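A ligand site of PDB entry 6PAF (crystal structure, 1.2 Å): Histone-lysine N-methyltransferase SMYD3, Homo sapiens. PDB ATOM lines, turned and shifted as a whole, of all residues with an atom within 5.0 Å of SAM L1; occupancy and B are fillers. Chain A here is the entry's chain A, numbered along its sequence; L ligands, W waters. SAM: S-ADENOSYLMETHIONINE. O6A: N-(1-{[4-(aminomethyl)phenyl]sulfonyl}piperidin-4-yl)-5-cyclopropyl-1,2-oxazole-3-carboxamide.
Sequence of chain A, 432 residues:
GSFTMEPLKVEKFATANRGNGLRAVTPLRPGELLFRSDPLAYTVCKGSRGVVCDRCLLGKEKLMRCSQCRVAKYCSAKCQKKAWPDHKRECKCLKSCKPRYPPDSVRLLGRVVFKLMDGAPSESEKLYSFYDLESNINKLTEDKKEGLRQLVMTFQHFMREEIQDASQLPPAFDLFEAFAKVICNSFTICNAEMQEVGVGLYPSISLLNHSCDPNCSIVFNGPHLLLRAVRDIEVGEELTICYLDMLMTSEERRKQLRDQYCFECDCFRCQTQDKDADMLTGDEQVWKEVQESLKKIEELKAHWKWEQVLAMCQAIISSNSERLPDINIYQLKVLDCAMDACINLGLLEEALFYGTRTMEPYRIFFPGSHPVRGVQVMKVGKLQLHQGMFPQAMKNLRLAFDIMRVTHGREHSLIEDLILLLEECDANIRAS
The backbone carbonyl oxygen of Tyr 261 lies within hydrogen-bond range of an oxygen (O3') of SAM L1, at 2.6 Å. OH of Tyr 128 is in hydrogen-bond range of O of SAM L1, at 2.7 Å. N of SAM L1 sits at hydrogen-bond distance from O of Arg 18 (2.7 Å). N of Asn 20 sits at hydrogen-bond distance from OXT of SAM L1, 2.8 Å away. N of SAM L1 sits at hydrogen-bond distance from O of Asn 20 (2.8 Å). The side-chain amide oxygen (OD1) of Asn 209 sits at hydrogen-bond distance from a nitrogen (N) of SAM L1. The backbone NH (N) of His 210 lies within hydrogen-bond range of a nitrogen (N7) of SAM L1 (2.9 Å). A nitrogen (N6) of SAM L1 lies within hydrogen-bond range of the backbone carbonyl oxygen of His 210 (2.9 Å). The side-chain amide nitrogen (ND2) of Asn 136 lies within hydrogen-bond range of an oxygen (O3') of SAM L1, 2.9 Å away. O of Tyr 243 lies close to N35 of O6A L2 (3.3 Å).
ND2 of Asn 136 is in hydrogen-bond range of O of Tyr 261 (3.4 Å). ND2 of Asn 20 sits at hydrogen-bond distance from OH of Tyr 128 (2.9 Å). The backbone carbonyl oxygen (O) of Asp 132 sits at hydrogen-bond distance from the side-chain hydroxyl (OH) of Tyr 128. O of Arg 18 lies within hydrogen-bond range of ND2 of Asn 209 (3.4 Å). A ring nitrogen (ND1) of His 210 sits at hydrogen-bond distance from the backbone NH (N) of Tyr 243. The side-chain amide nitrogen of Asn 136 lies within hydrogen-bond range of the side-chain sulfur of Cys 184. N of Asn 136 is in hydrogen-bond range of OE2 of Glu 134. The side-chain amide nitrogen (ND2) of Asn 185 sits at hydrogen-bond distance from the backbone carbonyl oxygen (O) of Glu 134.
OD1 of Asn 185 lies close to SD of SAM L1 (3.6 Å). O of Ser 206 sits close to SD of SAM L1 (3.4 Å). The side-chain hydroxyl of Tyr 243 lies close to a sulfur (SD) of SAM L1, at 3.7 Å. Gly 19 touches SAM L1 (C to OXT, 3.7 Å). Glu 134 touches SAM L1. O of Cys 184 touches CE of SAM L1 (3.5 Å). Leu 207 touches SAM L1. O of Leu 208 touches CG of SAM L1 (3.4 Å). Phe 263 touches SAM L1. Hydrophobic or aromatic side chains that line SAM L1: Tyr 128, His 210, Tyr 243, Tyr 261 and Phe 263. Of the 22 residues printed, 16 come within 4 Å of SAM L1.
Water W6 lies within hydrogen-bond range of O2' of SAM L1, O of Cys 262 and OD1 of Asn 136. Water W2 lies within hydrogen-bond range of OXT of SAM L1 (2.7 Å) and OE1 of Glu 134 (2.8 Å). Water W5 lies within hydrogen-bond range of O of SAM L1 (2.7 Å), OD1 of Asn 185 (2.8 Å) and N of Glu 134 (2.8 Å). Water W4 bridges the side-chain carboxylate of Glu 134 (2.8 Å) and a nitrogen (N) of SAM L1 (2.9 Å). Water W1 lies within hydrogen-bond range of the backbone carbonyl oxygen of Glu 264 (2.8 Å) and a nitrogen (N1) of SAM L1 (2.9 Å).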
ATOM      1  N   ASN A  17       3.960  -4.952   9.212  1.00  0.00           N
ATOM      2  CA  ASN A  17       4.101  -6.195   9.984  1.00  0.00           C
ATOM      3  C   ASN A  17       5.539  -6.522  10.387  1.00  0.00           C
ATOM      4  O   ASN A  17       5.837  -7.683  10.717  1.00  0.00           O
ATOM      5  CB  ASN A  17       3.476  -7.404   9.234  1.00  0.00           C
ATOM      6  CG  ASN A  17       4.102  -7.645   7.892  1.00  0.00           C
ATOM      7  OD1 ASN A  17       5.291  -7.400   7.691  1.00  0.00           O
ATOM      8  ND2 ASN A  17       3.307  -8.138   6.943  1.00  0.00           N
ATOM      9  N   ARG A  18       6.420  -5.542  10.384  1.00  0.00           N
ATOM     10  CA  ARG A  18       7.783  -5.795  10.830  1.00  0.00           C
ATOM     11  C   ARG A  18       8.288  -4.672  11.710  1.00  0.00           C
ATOM     12  O   ARG A  18       9.484  -4.358  11.687  1.00  0.00           O
ATOM     13  CB  ARG A  18       8.752  -6.144   9.703  1.00  0.00           C
ATOM     14  CG  ARG A  18       8.482  -5.480   8.429  1.00  0.00           C
ATOM     15  CD  ARG A  18       9.483  -5.940   7.370  1.00  0.00           C
ATOM     16  NE  ARG A  18       9.015  -6.931   6.420  1.00  0.00           N
ATOM     17  CZ  ARG A  18       9.481  -7.005   5.167  1.00  0.00           C
ATOM     18  NH1 ARG A  18      10.375  -6.115   4.754  1.00  0.00           N
ATOM     19  NH2 ARG A  18       9.044  -7.948   4.348  1.00  0.00           N
ATOM     20  N   GLY A  19       7.413  -4.089  12.493  1.00  0.00           N
ATOM     21  CA  GLY A  19       7.824  -3.056  13.432  1.00  0.00           C
ATOM     22  C   GLY A  19       8.179  -1.772  12.711  1.00  0.00           C
ATOM     23  O   GLY A  19       7.612  -1.425  11.676  1.00  0.00           O
ATOM     24  N   ASN A  20       9.129  -1.029  13.279  1.00  0.00           N
ATOM     25  CA  ASN A  20       9.625   0.125  12.563  1.00  0.00           C
ATOM     26  C   ASN A  20      10.592  -0.303  11.472  1.00  0.00           C
ATOM     27  O   ASN A  20      11.165  -1.380  11.515  1.00  0.00           O
ATOM     28  CB  ASN A  20      10.311   1.052  13.554  1.00  0.00           C
ATOM     29  CG  ASN A  20       9.348   1.582  14.542  1.00  0.00           C
ATOM     30  OD1 ASN A  20       8.271   2.029  14.175  1.00  0.00           O
ATOM     31  ND2 ASN A  20       9.687   1.498  15.814  1.00  0.00           N
ATOM     32  N   TYR A 128      16.914   6.865  15.704  1.00  0.00           N
ATOM     33  CA  TYR A 128      16.366   5.829  16.557  1.00  0.00           C
ATOM     34  C   TYR A 128      17.387   5.607  17.634  1.00  0.00           C
ATOM     35  O   TYR A 128      18.584   5.600  17.345  1.00  0.00           O
ATOM     36  CB  TYR A 128      16.268   4.542  15.742  1.00  0.00           C
ATOM     37  CG  TYR A 128      15.224   3.503  16.114  1.00  0.00           C
ATOM     38  CD1 TYR A 128      13.890   3.839  16.356  1.00  0.00           C
ATOM     39  CD2 TYR A 128      15.530   2.155  16.093  1.00  0.00           C
ATOM     40  CE1 TYR A 128      12.931   2.840  16.589  1.00  0.00           C
ATOM     41  CE2 TYR A 128      14.589   1.178  16.316  1.00  0.00           C
ATOM     42  CZ  TYR A 128      13.294   1.541  16.569  1.00  0.00           C
ATOM     43  OH  TYR A 128      12.339   0.596  16.726  1.00  0.00           O
ATOM     44  N   ASP A 132      14.709   3.051  22.033  1.00  0.00           N
ATOM     45  CA  ASP A 132      13.664   2.693  21.085  1.00  0.00           C
ATOM     46  C   ASP A 132      13.798   1.276  20.546  1.00  0.00           C
ATOM     47  O   ASP A 132      12.844   0.791  19.916  1.00  0.00           O
ATOM     48  CB  ASP A 132      13.743   3.607  19.841  1.00  0.00           C
ATOM     49  CG  ASP A 132      13.500   5.053  20.137  1.00  0.00           C
ATOM     50  OD1 ASP A 132      12.617   5.368  20.983  1.00  0.00           O
ATOM     51  OD2 ASP A 132      14.169   5.883  19.475  1.00  0.00           O
ATOM     52  N   LEU A 133      14.942   0.644  20.690  1.00  0.00           N
ATOM     53  CA  LEU A 133      15.206  -0.570  19.937  1.00  0.00           C
ATOM     54  C   LEU A 133      14.207  -1.667  20.280  1.00  0.00           C
ATOM     55  O   LEU A 133      13.755  -1.794  21.424  1.00  0.00           O
ATOM     56  CB  LEU A 133      16.582  -1.107  20.270  1.00  0.00           C
ATOM     57  CG  LEU A 133      17.743  -0.240  19.822  1.00  0.00           C
ATOM     58  CD1 LEU A 133      19.022  -0.868  20.307  1.00  0.00           C
ATOM     59  CD2 LEU A 133      17.795  -0.069  18.305  1.00  0.00           C
ATOM     60  N   GLU A 134      13.952  -2.515  19.307  1.00  0.00           N
ATOM     61  CA  GLU A 134      13.106  -3.696  19.487  1.00  0.00           C
ATOM     62  C   GLU A 134      13.768  -4.677  20.443  1.00  0.00           C
ATOM     63  O   GLU A 134      14.960  -4.951  20.331  1.00  0.00           O
ATOM     64  CB  GLU A 134      12.946  -4.366  18.127  1.00  0.00           C
ATOM     65  CG  GLU A 134      12.152  -5.671  18.198  1.00  0.00           C
ATOM     66  CD  GLU A 134      10.753  -5.413  18.569  1.00  0.00           C
ATOM     67  OE1 GLU A 134      10.011  -4.882  17.708  1.00  0.00           O
ATOM     68  OE2 GLU A 134      10.377  -5.751  19.734  1.00  0.00           O
ATOM     69  N   ASN A 136      11.846  -7.674  21.301  1.00  0.00           N
ATOM     70  CA  ASN A 136      11.192  -8.950  21.049  1.00  0.00           C
ATOM     71  C   ASN A 136      10.869  -9.716  22.329  1.00  0.00           C
ATOM     72  O   ASN A 136      10.761 -10.935  22.303  1.00  0.00           O
ATOM     73  CB  ASN A 136      11.999  -9.815  20.103  1.00  0.00           C
ATOM     74  CG  ASN A 136      11.861  -9.325  18.710  1.00  0.00           C
ATOM     75  OD1 ASN A 136      10.759  -9.000  18.284  1.00  0.00           O
ATOM     76  ND2 ASN A 136      12.972  -9.142  18.012  1.00  0.00           N
ATOM     77  N   CYS A 184      19.105  -8.759  19.269  1.00  0.00           N
ATOM     78  CA  CYS A 184      18.496  -8.547  17.964  1.00  0.00           C
ATOM     79  C   CYS A 184      18.921  -7.248  17.284  1.00  0.00           C
ATOM     80  O   CYS A 184      18.330  -6.882  16.269  1.00  0.00           O
ATOM     81  CB  CYS A 184      16.983  -8.708  17.980  1.00  0.00           C
ATOM     82  SG  CYS A 184      16.107  -7.532  18.988  1.00  0.00           S
ATOM     83  N   ASN A 185      19.955  -6.600  17.790  1.00  0.00           N
ATOM     84  CA  ASN A 185      20.401  -5.325  17.240  1.00  0.00           C
ATOM     85  C   ASN A 185      21.923  -5.228  17.174  1.00  0.00           C
ATOM     86  O   ASN A 185      22.448  -4.151  16.971  1.00  0.00           O
ATOM     87  CB  ASN A 185      19.849  -4.140  18.046  1.00  0.00           C
ATOM     88  CG  ASN A 185      18.387  -3.961  17.821  1.00  0.00           C
ATOM     89  OD1 ASN A 185      17.972  -3.436  16.804  1.00  0.00           O
ATOM     90  ND2 ASN A 185      17.572  -4.408  18.780  1.00  0.00           N
ATOM     91  N   SER A 206      19.812   0.338  13.074  1.00  0.00           N
ATOM     92  CA  SER A 206      18.929  -0.707  13.546  1.00  0.00           C
ATOM     93  C   SER A 206      17.531  -0.569  13.019  1.00  0.00           C
ATOM     94  O   SER A 206      16.756  -1.515  13.196  1.00  0.00           O
ATOM     95  CB  SER A 206      18.849  -0.741  15.056  1.00  0.00           C
ATOM     96  OG  SER A 206      19.830  -1.612  15.602  1.00  0.00           O
ATOM     97  N   LEU A 207      17.137   0.529  12.412  1.00  0.00           N
ATOM     98  CA  LEU A 207      15.814   0.587  11.787  1.00  0.00           C
ATOM     99  C   LEU A 207      15.688  -0.334  10.601  1.00  0.00           C
ATOM    100  O   LEU A 207      14.552  -0.717  10.261  1.00  0.00           O
ATOM    101  CB  LEU A 207      15.523   2.011  11.324  1.00  0.00           C
ATOM    102  CG  LEU A 207      15.056   2.917  12.464  1.00  0.00           C
ATOM    103  CD1 LEU A 207      15.069   4.372  12.047  1.00  0.00           C
ATOM    104  CD2 LEU A 207      13.656   2.547  12.955  1.00  0.00           C
ATOM    105  N   LEU A 208      16.791  -0.707   9.952  1.00  0.00           N
ATOM    106  CA  LEU A 208      16.654  -1.510   8.747  1.00  0.00           C
ATOM    107  C   LEU A 208      16.186  -2.903   9.060  1.00  0.00           C
ATOM    108  O   LEU A 208      16.815  -3.645   9.815  1.00  0.00           O
ATOM    109  CB  LEU A 208      18.003  -1.626   8.042  1.00  0.00           C
ATOM    110  CG  LEU A 208      18.481  -0.289   7.458  1.00  0.00           C
ATOM    111  CD1 LEU A 208      19.994  -0.272   7.421  1.00  0.00           C
ATOM    112  CD2 LEU A 208      18.004  -0.155   6.081  1.00  0.00           C
ATOM    113  N   ASN A 209      15.132  -3.307   8.381  1.00  0.00           N
ATOM    114  CA  ASN A 209      14.708  -4.690   8.430  1.00  0.00           C
ATOM    115  C   ASN A 209      15.507  -5.548   7.461  1.00  0.00           C
ATOM    116  O   ASN A 209      16.221  -5.049   6.576  1.00  0.00           O
ATOM    117  CB  ASN A 209      13.192  -4.776   8.182  1.00  0.00           C
ATOM    118  CG  ASN A 209      12.428  -4.258   9.362  1.00  0.00           C
ATOM    119  OD1 ASN A 209      12.702  -4.640  10.501  1.00  0.00           O
ATOM    120  ND2 ASN A 209      11.485  -3.359   9.133  1.00  0.00           N
ATOM    121  N   HIS A 210      15.386  -6.839   7.656  1.00  0.00           N
ATOM    122  CA  HIS A 210      16.175  -7.835   6.950  1.00  0.00           C
ATOM    123  C   HIS A 210      15.501  -8.272   5.661  1.00  0.00           C
ATOM    124  O   HIS A 210      14.266  -8.437   5.612  1.00  0.00           O
ATOM    125  CB  HIS A 210      16.281  -9.071   7.842  1.00  0.00           C
ATOM    126  CG  HIS A 210      16.780 -10.278   7.109  1.00  0.00           C
ATOM    127  ND1 HIS A 210      18.123 -10.529   6.894  1.00  0.00           N
ATOM    128  CD2 HIS A 210      16.089 -11.269   6.501  1.00  0.00           C
ATOM    129  CE1 HIS A 210      18.235 -11.630   6.180  1.00  0.00           C
ATOM    130  NE2 HIS A 210      17.012 -12.090   5.919  1.00  0.00           N
ATOM    131  N   TYR A 243      20.846  -9.491   7.162  1.00  0.00           N
ATOM    132  CA  TYR A 243      21.513  -9.616   8.429  1.00  0.00           C
ATOM    133  C   TYR A 243      22.536 -10.738   8.446  1.00  0.00           C
ATOM    134  O   TYR A 243      23.266 -10.853   9.414  1.00  0.00           O
ATOM    135  CB  TYR A 243      20.500  -9.916   9.537  1.00  0.00           C
ATOM    136  CG  TYR A 243      19.503  -8.827   9.865  1.00  0.00           C
ATOM    137  CD1 TYR A 243      19.472  -7.586   9.214  1.00  0.00           C
ATOM    138  CD2 TYR A 243      18.539  -9.093  10.827  1.00  0.00           C
ATOM    139  CE1 TYR A 243      18.505  -6.643   9.563  1.00  0.00           C
ATOM    140  CE2 TYR A 243      17.602  -8.155  11.191  1.00  0.00           C
ATOM    141  CZ  TYR A 243      17.583  -6.942  10.535  1.00  0.00           C
ATOM    142  OH  TYR A 243      16.587  -6.043  10.897  1.00  0.00           O
ATOM    143  N   TYR A 261      16.592 -13.291  15.978  1.00  0.00           N
ATOM    144  CA  TYR A 261      15.772 -12.145  15.589  1.00  0.00           C
ATOM    145  C   TYR A 261      14.277 -12.355  15.801  1.00  0.00           C
ATOM    146  O   TYR A 261      13.497 -11.405  15.524  1.00  0.00           O
ATOM    147  CB  TYR A 261      16.085 -11.754  14.141  1.00  0.00           C
ATOM    148  CG  TYR A 261      17.528 -11.292  13.988  1.00  0.00           C
ATOM    149  CD1 TYR A 261      17.922 -10.059  14.516  1.00  0.00           C
ATOM    150  CD2 TYR A 261      18.491 -12.096  13.405  1.00  0.00           C
ATOM    151  CE1 TYR A 261      19.229  -9.630  14.453  1.00  0.00           C
ATOM    152  CE2 TYR A 261      19.815 -11.646  13.318  1.00  0.00           C
ATOM    153  CZ  TYR A 261      20.143 -10.442  13.863  1.00  0.00           C
ATOM    154  OH  TYR A 261      21.448  -9.950  13.815  1.00  0.00           O
ATOM    155  N   CYS A 262      13.849 -13.528  16.220  1.00  0.00           N
ATOM    156  CA  CYS A 262      12.418 -13.776  16.464  1.00  0.00           C
ATOM    157  C   CYS A 262      11.536 -13.401  15.279  1.00  0.00           C
ATOM    158  O   CYS A 262      10.481 -12.792  15.470  1.00  0.00           O
ATOM    159  CB  CYS A 262      11.907 -13.078  17.718  1.00  0.00           C
ATOM    160  SG  CYS A 262      12.740 -13.653  19.222  1.00  0.00           S
ATOM    161  N   PHE A 263      11.871 -13.827  14.062  1.00  0.00           N
ATOM    162  CA  PHE A 263      10.906 -13.687  12.993  1.00  0.00           C
ATOM    163  C   PHE A 263      11.093 -14.806  11.990  1.00  0.00           C
ATOM    164  O   PHE A 263      12.136 -15.462  11.952  1.00  0.00           O
ATOM    165  CB  PHE A 263      10.901 -12.291  12.319  1.00  0.00           C
ATOM    166  CG  PHE A 263      12.074 -12.027  11.420  1.00  0.00           C
ATOM    167  CD1 PHE A 263      13.233 -11.543  11.928  1.00  0.00           C
ATOM    168  CD2 PHE A 263      11.994 -12.288  10.061  1.00  0.00           C
ATOM    169  CE1 PHE A 263      14.312 -11.268  11.079  1.00  0.00           C
ATOM    170  CE2 PHE A 263      13.056 -12.048   9.194  1.00  0.00           C
ATOM    171  CZ  PHE A 263      14.203 -11.574   9.717  1.00  0.00           C
ATOM    172  N   GLU A 264      10.035 -15.009  11.190  1.00  0.00           N
ATOM    173  CA  GLU A 264       9.920 -15.990  10.110  1.00  0.00           C
ATOM    174  C   GLU A 264       9.992 -15.172   8.826  1.00  0.00           C
ATOM    175  O   GLU A 264       9.239 -14.195   8.674  1.00  0.00           O
ATOM    176  CB  GLU A 264       8.532 -16.683  10.207  1.00  0.00           C
ATOM    177  CG  GLU A 264       8.054 -17.019  11.650  1.00  0.00           C
ATOM    178  CD  GLU A 264       8.949 -18.067  12.285  1.00  0.00           C
ATOM    179  OE1 GLU A 264       8.844 -18.348  13.494  1.00  0.00           O
ATOM    180  OE2 GLU A 264       9.783 -18.652  11.559  1.00  0.00           O
ATOM    181  N   CYS A 265      10.933 -15.500   7.952  1.00  0.00           N
ATOM    182  CA  CYS A 265      11.217 -14.648   6.792  1.00  0.00           C
ATOM    183  C   CYS A 265      10.307 -15.063   5.679  1.00  0.00           C
ATOM    184  O   CYS A 265      10.244 -16.247   5.323  1.00  0.00           O
ATOM    185  CB  CYS A 265      12.639 -14.754   6.271  1.00  0.00           C
ATOM    186  SG  CYS A 265      13.125 -13.508   4.977  1.00  0.00           S
HETATM  187  N   SAM L   1      11.722  -3.666  13.001  1.00  0.00           N
HETATM  188  CA  SAM L   1      12.792  -3.244  13.935  1.00  0.00           C
HETATM  189  C   SAM L   1      12.275  -2.258  14.932  1.00  0.00           C
HETATM  190  O   SAM L   1      13.105  -1.741  15.665  1.00  0.00           O
HETATM  191  OXT SAM L   1      11.063  -2.046  14.965  1.00  0.00           O
HETATM  192  CB  SAM L   1      14.024  -2.743  13.175  1.00  0.00           C
HETATM  193  CG  SAM L   1      14.959  -3.866  12.702  1.00  0.00           C
HETATM  194  SD  SAM L   1      15.771  -4.588  14.193  1.00  0.00           S
HETATM  195  CE  SAM L   1      17.530  -4.538  13.797  1.00  0.00           C
HETATM  196  C5' SAM L   1      15.530  -6.397  14.064  1.00  0.00           C
HETATM  197  C4' SAM L   1      14.099  -6.837  14.313  1.00  0.00           C
HETATM  198  O4' SAM L   1      13.228  -6.323  13.284  1.00  0.00           O
HETATM  199  C3' SAM L   1      13.959  -8.360  14.255  1.00  0.00           C
HETATM  200  O3' SAM L   1      14.405  -8.923  15.454  1.00  0.00           O
HETATM  201  C2' SAM L   1      12.469  -8.476  13.974  1.00  0.00           C
HETATM  202  O2' SAM L   1      11.750  -8.163  15.161  1.00  0.00           O
HETATM  203  C1' SAM L   1      12.276  -7.343  12.993  1.00  0.00           C
HETATM  204  N9  SAM L   1      12.550  -7.764  11.620  1.00  0.00           N
HETATM  205  C8  SAM L   1      13.645  -7.450  10.831  1.00  0.00           C
HETATM  206  N7  SAM L   1      13.493  -7.923   9.600  1.00  0.00           N
HETATM  207  C5  SAM L   1      12.278  -8.504   9.536  1.00  0.00           C
HETATM  208  C6  SAM L   1      11.583  -9.140   8.523  1.00  0.00           C
HETATM  209  N6  SAM L   1      12.026  -9.298   7.272  1.00  0.00           N
HETATM  210  N1  SAM L   1      10.343  -9.650   8.800  1.00  0.00           N
HETATM  211  C2  SAM L   1       9.833  -9.521  10.054  1.00  0.00           C
HETATM  212  N3  SAM L   1      10.461  -8.914  11.084  1.00  0.00           N
HETATM  213  C4  SAM L   1      11.670  -8.390  10.792  1.00  0.00           C
HETATM  214  C27 O6A L   2      26.532  -8.975   8.912  1.00  0.00           C
HETATM  215  C29 O6A L   2      25.961  -9.828   7.771  1.00  0.00           C
HETATM  216  C12 O6A L   2      30.173 -11.038   5.942  1.00  0.00           C
HETATM  217  C24 O6A L   2      27.593  -7.974   8.430  1.00  0.00           C
HETATM  218  C32 O6A L   2      27.073 -10.552   7.058  1.00  0.00           C
HETATM  219  N01 O6A L   2      32.908 -15.148   6.872  1.00  0.00           N
HETATM  220  C04 O6A L   2      33.039 -13.784   7.402  1.00  0.00           C
HETATM  221  C07 O6A L   2      31.983 -12.842   6.856  1.00  0.00           C
HETATM  222  C08 O6A L   2      30.717 -13.313   6.454  1.00  0.00           C
HETATM  223  C10 O6A L   2      29.798 -12.373   5.986  1.00  0.00           C
HETATM  224  C13 O6A L   2      31.414 -10.544   6.321  1.00  0.00           C
HETATM  225  C15 O6A L   2      32.312 -11.487   6.782  1.00  0.00           C
HETATM  226  S17 O6A L   2      29.013  -9.842   5.365  1.00  0.00           S
HETATM  227  O18 O6A L   2      28.142 -10.402   4.366  1.00  0.00           O
HETATM  228  O19 O6A L   2      29.710  -8.642   4.999  1.00  0.00           O
HETATM  229  N20 O6A L   2      28.029  -9.508   6.657  1.00  0.00           N
HETATM  230  C21 O6A L   2      28.683  -8.778   7.760  1.00  0.00           C
HETATM  231  N35 O6A L   2      25.364  -8.247   9.348  1.00  0.00           N
HETATM  232  C37 O6A L   2      25.181  -7.873  10.626  1.00  0.00           C
HETATM  233  O38 O6A L   2      25.983  -8.088  11.504  1.00  0.00           O
HETATM  234  C39 O6A L   2      23.930  -7.194  10.811  1.00  0.00           C
HETATM  235  C40 O6A L   2      23.182  -7.014  12.033  1.00  0.00           C
HETATM  236  C42 O6A L   2      22.088  -6.317  11.647  1.00  0.00           C
HETATM  237  O43 O6A L   2      22.122  -6.059  10.313  1.00  0.00           O
HETATM  238  N44 O6A L   2      23.260  -6.592   9.829  1.00  0.00           N
HETATM  239  C45 O6A L   2      20.953  -5.766  12.400  1.00  0.00           C
HETATM  240  C47 O6A L   2      21.179  -5.201  13.735  1.00  0.00           C
HETATM  241  C50 O6A L   2      20.504  -6.521  13.572  1.00  0.00           C
HETATM  242  O   HOH W   1       9.034 -11.813   7.297  1.00  0.00           O
HETATM  243  O   HOH W   2       9.820  -2.077  17.383  1.00  0.00           O
HETATM  244  O   HOH W   3       8.630  -9.206  13.225  1.00  0.00           O
HETATM  245  O   HOH W   4      10.394  -5.353  14.961  1.00  0.00           O
HETATM  246  O   HOH W   5      15.470  -2.265  16.930  1.00  0.00           O
HETATM  247  O   HOH W   6      10.038 -10.156  15.575  1.00  0.00           O
HETATM  248  O   HOH W   7      19.304  -3.190  11.123  1.00  0.00           O
HETATM  249  O   HOH W   8      11.042 -10.966   5.035  1.00  0.00           O
